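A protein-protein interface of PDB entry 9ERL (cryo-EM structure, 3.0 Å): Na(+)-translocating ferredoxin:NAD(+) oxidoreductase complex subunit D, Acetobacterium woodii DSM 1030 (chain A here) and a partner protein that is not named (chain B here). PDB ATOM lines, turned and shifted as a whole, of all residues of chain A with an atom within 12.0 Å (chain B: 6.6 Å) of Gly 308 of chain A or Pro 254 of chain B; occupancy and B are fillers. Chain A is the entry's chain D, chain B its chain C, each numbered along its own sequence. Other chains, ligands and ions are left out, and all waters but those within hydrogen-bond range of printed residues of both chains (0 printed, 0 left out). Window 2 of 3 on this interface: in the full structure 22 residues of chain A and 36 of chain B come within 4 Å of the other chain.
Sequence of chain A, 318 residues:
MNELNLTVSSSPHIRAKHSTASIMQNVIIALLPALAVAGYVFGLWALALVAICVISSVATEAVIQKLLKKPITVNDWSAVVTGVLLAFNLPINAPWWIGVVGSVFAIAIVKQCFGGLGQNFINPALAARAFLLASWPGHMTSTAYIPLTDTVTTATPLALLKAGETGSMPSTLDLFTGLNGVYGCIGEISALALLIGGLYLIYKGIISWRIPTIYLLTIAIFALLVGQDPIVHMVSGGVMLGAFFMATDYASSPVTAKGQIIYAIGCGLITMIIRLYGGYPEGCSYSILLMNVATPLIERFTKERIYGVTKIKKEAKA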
ATOM      1  N   GLU A 304      15.428 -19.528  13.607  1.00  0.00           N
ATOM      2  CA  GLU A 304      16.320 -18.425  13.916  1.00  0.00           C
ATOM      3  C   GLU A 304      15.821 -17.665  15.145  1.00  0.00           C
ATOM      4  O   GLU A 304      14.794 -17.998  15.742  1.00  0.00           O
ATOM      5  CB  GLU A 304      16.457 -17.502  12.706  1.00  0.00           C
ATOM      6  CG  GLU A 304      17.874 -17.017  12.463  1.00  0.00           C
ATOM      7  CD  GLU A 304      17.961 -16.011  11.335  1.00  0.00           C
ATOM      8  OE1 GLU A 304      17.073 -16.024  10.458  1.00  0.00           O
ATOM      9  OE2 GLU A 304      18.920 -15.212  11.323  1.00  0.00           O
ATOM     10  N   ARG A 305      16.559 -16.628  15.528  1.00  0.00           N
ATOM     11  CA  ARG A 305      16.260 -15.846  16.719  1.00  0.00           C
ATOM     12  C   ARG A 305      15.608 -14.530  16.316  1.00  0.00           C
ATOM     13  O   ARG A 305      16.120 -13.821  15.444  1.00  0.00           O
ATOM     14  CB  ARG A 305      17.531 -15.587  17.530  1.00  0.00           C
ATOM     15  CG  ARG A 305      17.287 -15.015  18.916  1.00  0.00           C
ATOM     16  CD  ARG A 305      18.567 -14.466  19.526  1.00  0.00           C
ATOM     17  NE  ARG A 305      19.098 -13.344  18.763  1.00  0.00           N
ATOM     18  CZ  ARG A 305      18.831 -12.071  19.018  1.00  0.00           C
ATOM     19  NH1 ARG A 305      18.046 -11.717  20.022  1.00  0.00           N
ATOM     20  NH2 ARG A 305      19.364 -11.128  18.245  1.00  0.00           N
ATOM     21  N   ILE A 306      14.481 -14.209  16.956  1.00  0.00           N
ATOM     22  CA  ILE A 306      13.751 -12.993  16.620  1.00  0.00           C
ATOM     23  C   ILE A 306      14.516 -11.769  17.115  1.00  0.00           C
ATOM     24  O   ILE A 306      15.318 -11.832  18.053  1.00  0.00           O
ATOM     25  CB  ILE A 306      12.328 -13.038  17.203  1.00  0.00           C
ATOM     26  CG1 ILE A 306      11.775 -14.462  17.160  1.00  0.00           C
ATOM     27  CG2 ILE A 306      11.392 -12.117  16.437  1.00  0.00           C
ATOM     28  CD1 ILE A 306      11.455 -14.955  15.765  1.00  0.00           C
ATOM     29  N   TYR A 307      14.270 -10.639  16.458  1.00  0.00           N
ATOM     30  CA  TYR A 307      14.883  -9.375  16.844  1.00  0.00           C
ATOM     31  C   TYR A 307      14.338  -8.936  18.198  1.00  0.00           C
ATOM     32  O   TYR A 307      13.120  -8.889  18.399  1.00  0.00           O
ATOM     33  CB  TYR A 307      14.605  -8.321  15.771  1.00  0.00           C
ATOM     34  CG  TYR A 307      15.184  -6.944  16.033  1.00  0.00           C
ATOM     35  CD1 TYR A 307      14.521  -6.023  16.834  1.00  0.00           C
ATOM     36  CD2 TYR A 307      16.383  -6.556  15.454  1.00  0.00           C
ATOM     37  CE1 TYR A 307      15.046  -4.776  17.072  1.00  0.00           C
ATOM     38  CE2 TYR A 307      16.912  -5.303  15.682  1.00  0.00           C
ATOM     39  CZ  TYR A 307      16.237  -4.417  16.491  1.00  0.00           C
ATOM     40  OH  TYR A 307      16.758  -3.167  16.722  1.00  0.00           O
ATOM     41  N   GLY A 308      15.236  -8.609  19.125  1.00  0.00           N
ATOM     42  CA  GLY A 308      14.865  -8.081  20.422  1.00  0.00           C
ATOM     43  C   GLY A 308      14.545  -9.123  21.470  1.00  0.00           C
ATOM     44  O   GLY A 308      14.158  -8.751  22.585  1.00  0.00           O
ATOM     45  N   VAL A 309      14.683 -10.408  21.158  1.00  0.00           N
ATOM     46  CA  VAL A 309      14.370 -11.486  22.090  1.00  0.00           C
ATOM     47  C   VAL A 309      15.669 -11.998  22.694  1.00  0.00           C
ATOM     48  O   VAL A 309      16.589 -12.396  21.967  1.00  0.00           O
ATOM     49  CB  VAL A 309      13.596 -12.616  21.391  1.00  0.00           C
ATOM     50  CG1 VAL A 309      13.732 -13.922  22.158  1.00  0.00           C
ATOM     51  CG2 VAL A 309      12.133 -12.237  21.235  1.00  0.00           C
ATOM     52  N   THR A 310      15.755 -11.973  24.025  1.00  0.00           N
ATOM     53  CA  THR A 310      16.904 -12.504  24.744  1.00  0.00           C
ATOM     54  C   THR A 310      16.670 -13.904  25.296  1.00  0.00           C
ATOM     55  O   THR A 310      17.570 -14.451  25.944  1.00  0.00           O
ATOM     56  CB  THR A 310      17.295 -11.569  25.896  1.00  0.00           C
ATOM     57  OG1 THR A 310      16.112 -11.058  26.523  1.00  0.00           O
ATOM     58  CG2 THR A 310      18.133 -10.411  25.378  1.00  0.00           C
ATOM     59  N   LYS A 311      15.476 -14.471  25.075  1.00  0.00           N
ATOM     60  CA  LYS A 311      15.099 -15.847  25.401  1.00  0.00           C
ATOM     61  C   LYS A 311      14.970 -16.094  26.902  1.00  0.00           C
ATOM     62  O   LYS A 311      15.729 -15.546  27.708  1.00  0.00           O
ATOM     63  CB  LYS A 311      16.077 -16.855  24.783  1.00  0.00           C
ATOM     64  CG  LYS A 311      16.310 -16.669  23.292  1.00  0.00           C
ATOM     65  CD  LYS A 311      15.727 -17.826  22.500  1.00  0.00           C
ATOM     66  CE  LYS A 311      15.685 -17.512  21.015  1.00  0.00           C
ATOM     67  NZ  LYS A 311      14.403 -17.934  20.388  1.00  0.00           N
ATOM     68  N   ILE A 312      13.998 -16.922  27.277  1.00  0.00           N
ATOM     69  CA  ILE A 312      13.772 -17.326  28.659  1.00  0.00           C
ATOM     70  C   ILE A 312      14.189 -18.784  28.798  1.00  0.00           C
ATOM     71  O   ILE A 312      13.823 -19.624  27.968  1.00  0.00           O
ATOM     72  CB  ILE A 312      12.299 -17.121  29.069  1.00  0.00           C
ATOM     73  CG1 ILE A 312      11.954 -15.630  29.077  1.00  0.00           C
ATOM     74  CG2 ILE A 312      12.020 -17.733  30.431  1.00  0.00           C
ATOM     75  CD1 ILE A 312      10.523 -15.330  28.690  1.00  0.00           C
ATOM     76  N   LYS B 242      14.587   1.433  14.009  1.00  0.00           N
ATOM     77  CA  LYS B 242      15.056   0.242  14.703  1.00  0.00           C
ATOM     78  C   LYS B 242      16.312  -0.317  14.051  1.00  0.00           C
ATOM     79  O   LYS B 242      17.306  -0.601  14.730  1.00  0.00           O
ATOM     80  CB  LYS B 242      13.941  -0.809  14.724  1.00  0.00           C
ATOM     81  CG  LYS B 242      13.910  -1.661  15.968  1.00  0.00           C
ATOM     82  CD  LYS B 242      12.603  -2.430  16.081  1.00  0.00           C
ATOM     83  CE  LYS B 242      11.515  -1.592  16.720  1.00  0.00           C
ATOM     84  NZ  LYS B 242      10.329  -2.416  17.072  1.00  0.00           N
ATOM     85  N   GLU B 252      19.850  -3.249  20.615  1.00  0.00           N
ATOM     86  CA  GLU B 252      18.588  -3.775  20.115  1.00  0.00           C
ATOM     87  C   GLU B 252      17.465  -3.368  21.055  1.00  0.00           C
ATOM     88  O   GLU B 252      17.580  -3.534  22.273  1.00  0.00           O
ATOM     89  CB  GLU B 252      18.635  -5.301  19.984  1.00  0.00           C
ATOM     90  CG  GLU B 252      19.227  -5.801  18.680  1.00  0.00           C
ATOM     91  CD  GLU B 252      18.871  -7.248  18.400  1.00  0.00           C
ATOM     92  OE1 GLU B 252      18.160  -7.856  19.226  1.00  0.00           O
ATOM     93  OE2 GLU B 252      19.302  -7.776  17.355  1.00  0.00           O
ATOM     94  N   VAL B 253      16.391  -2.832  20.491  1.00  0.00           N
ATOM     95  CA  VAL B 253      15.203  -2.504  21.289  1.00  0.00           C
ATOM     96  C   VAL B 253      14.534  -3.800  21.737  1.00  0.00           C
ATOM     97  O   VAL B 253      14.348  -4.710  20.911  1.00  0.00           O
ATOM     98  CB  VAL B 253      14.241  -1.637  20.476  1.00  0.00           C
ATOM     99  CG1 VAL B 253      13.077  -1.178  21.336  1.00  0.00           C
ATOM    100  CG2 VAL B 253      14.973  -0.443  19.888  1.00  0.00           C
ATOM    101  N   PRO B 254      14.165  -3.940  23.019  1.00  0.00           N
ATOM    102  CA  PRO B 254      13.529  -5.185  23.479  1.00  0.00           C
ATOM    103  C   PRO B 254      12.171  -5.449  22.845  1.00  0.00           C
ATOM    104  O   PRO B 254      11.653  -4.622  22.089  1.00  0.00           O
ATOM    105  CB  PRO B 254      13.404  -4.973  24.993  1.00  0.00           C
ATOM    106  CG  PRO B 254      14.443  -3.960  25.321  1.00  0.00           C
ATOM    107  CD  PRO B 254      14.489  -3.044  24.141  1.00  0.00           C
ATOM    108  N   SER B 255      11.589  -6.605  23.151  1.00  0.00           N
ATOM    109  CA  SER B 255      10.333  -7.040  22.539  1.00  0.00           C
ATOM    110  C   SER B 255       9.186  -6.228  23.126  1.00  0.00           C
ATOM    111  O   SER B 255       8.651  -6.538  24.190  1.00  0.00           O
ATOM    112  CB  SER B 255      10.124  -8.534  22.752  1.00  0.00           C
ATOM    113  OG  SER B 255       9.113  -9.033  21.896  1.00  0.00           O
ATOM    114  N   GLY B 256       8.805  -5.168  22.415  1.00  0.00           N
ATOM    115  CA  GLY B 256       7.699  -4.328  22.831  1.00  0.00           C
ATOM    116  C   GLY B 256       8.028  -3.455  24.023  1.00  0.00           C
ATOM    117  O   GLY B 256       7.372  -3.550  25.065  1.00  0.00           O
ATOM    118  N   ALA B 257       9.042  -2.598  23.888  1.00  0.00           N
ATOM    119  CA  ALA B 257       9.485  -1.786  25.011  1.00  0.00           C
ATOM    120  C   ALA B 257       9.860  -0.355  24.650  1.00  0.00           C
ATOM    121  O   ALA B 257      10.338   0.365  25.532  1.00  0.00           O
ATOM    122  CB  ALA B 257      10.679  -2.457  25.708  1.00  0.00           C
ATOM    123  N   LEU B 258       9.679   0.074  23.389  1.00  0.00           N
ATOM    124  CA  LEU B 258       9.931   1.424  22.877  1.00  0.00           C
ATOM    125  C   LEU B 258      11.419   1.773  22.884  1.00  0.00           C
ATOM    126  O   LEU B 258      12.194   1.193  23.654  1.00  0.00           O
ATOM    127  CB  LEU B 258       9.130   2.464  23.674  1.00  0.00           C
ATOM    128  CG  LEU B 258       7.614   2.263  23.738  1.00  0.00           C
ATOM    129  CD1 LEU B 258       6.976   3.302  24.641  1.00  0.00           C
ATOM    130  CD2 LEU B 258       7.003   2.310  22.349  1.00  0.00           C
ATOM    131  N   PRO B 259      11.864   2.698  22.025  1.00  0.00           N
ATOM    132  CA  PRO B 259      13.297   3.046  21.998  1.00  0.00           C
ATOM    133  C   PRO B 259      13.810   3.694  23.272  1.00  0.00           C
ATOM    134  O   PRO B 259      15.025   3.684  23.501  1.00  0.00           O
ATOM    135  CB  PRO B 259      13.403   4.009  20.807  1.00  0.00           C
ATOM    136  CG  PRO B 259      12.232   3.696  19.957  1.00  0.00           C
ATOM    137  CD  PRO B 259      11.136   3.290  20.890  1.00  0.00           C
ATOM    138  N   ASP B 261      13.715   2.660  26.221  1.00  0.00           N
ATOM    139  CA  ASP B 261      14.372   1.665  27.056  1.00  0.00           C
ATOM    140  C   ASP B 261      15.757   1.288  26.550  1.00  0.00           C
ATOM    141  O   ASP B 261      16.489   0.594  27.263  1.00  0.00           O
ATOM    142  CB  ASP B 261      13.506   0.409  27.163  1.00  0.00           C
ATOM    143  CG  ASP B 261      12.224   0.653  27.927  1.00  0.00           C
ATOM    144  OD1 ASP B 261      11.992   1.806  28.342  1.00  0.00           O
ATOM    145  OD2 ASP B 261      11.450  -0.307  28.116  1.00  0.00           O
ATOM    146  N   ALA B 262      16.129   1.716  25.347  1.00  0.00           N
ATOM    147  CA  ALA B 262      17.476   1.512  24.835  1.00  0.00           C
ATOM    148  C   ALA B 262      18.396   2.690  25.123  1.00  0.00           C
ATOM    149  O   ALA B 262      19.576   2.641  24.760  1.00  0.00           O
ATOM    150  CB  ALA B 262      17.437   1.242  23.328  1.00  0.00           C
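Glu 304 of chain A touches none of the printed residues of chain B.
Printed residues of chain B within 4 Å of Arg 305 of chain A: Glu 252.
Of the printed residues of chain B, Tyr 307 of chain A touches Lys 242 (3.3 Å), Glu 252 (3.7 Å) and Val 253 (3.8 Å).
Gly 308 of chain A touches just these residues of chain B: Glu 252, Val 253, Pro 254 and Ser 255.
Of the printed residues of chain A, Lys 242 of chain B touches Tyr 307 (3.3 Å).
Of chain A, only Arg 305 (3.5 Å), Tyr 307 (3.7 Å) and Gly 308 (3.0 Å) come within 4 Å of Glu 252 of chain B.
Of chain A, only Gly 308 comes within 4 Å of Pro 254 of chain B.
No residue of chain A comes within 4 Å of Gly 256 of chain B.
No residue of chain A comes within 4 Å of Ala 257 of chain B.
No residue of chain A comes within 4 Å of Asp 261 of chain B.
The backbone carbonyl oxygen (O) of Val 309 of chain A lies within hydrogen-bond range of the guanidinium group (NH1) of Arg 305 of chain A.
The backbone carbonyl oxygen (O) of Lys 242 of chain B is in hydrogen-bond range of the side-chain hydroxyl (OH) of Tyr 307 of chain A (3.3 Å).
NH2 of Arg 305 of chain A lies within salt-bridge range of OE2 of Glu 252 of chain B, at 3.5 Å.
OE1 of Glu 252 of chain B is in hydrogen-bond range of N of Gly 308 of chain A (3.0 Å).
The backbone NH of Ser 255 of chain B lies within hydrogen-bond range of the backbone carbonyl oxygen of Gly 308 of chain A, at 3.4 Å.
Of the 11 printed residues of chain B, 5 touch a printed residue of chain A.
Hydrophobic or aromatic side chains of chain A within 4 Å of the printed part of chain B: Tyr 307.
Among the printed residues, 8 pairs touch across the chains.
Among the printed residues, merely in contact across the chains: Tyr 307 of chain A with Glu 252 of chain B (3.7 Å), Tyr 307 of chain A with Val 253 of chain B (3.8 Å), Gly 308 of chain A with Val 253 of chain B (3.4 Å) and Gly 308 of chain A with Pro 254 of chain B (3.7 Å).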
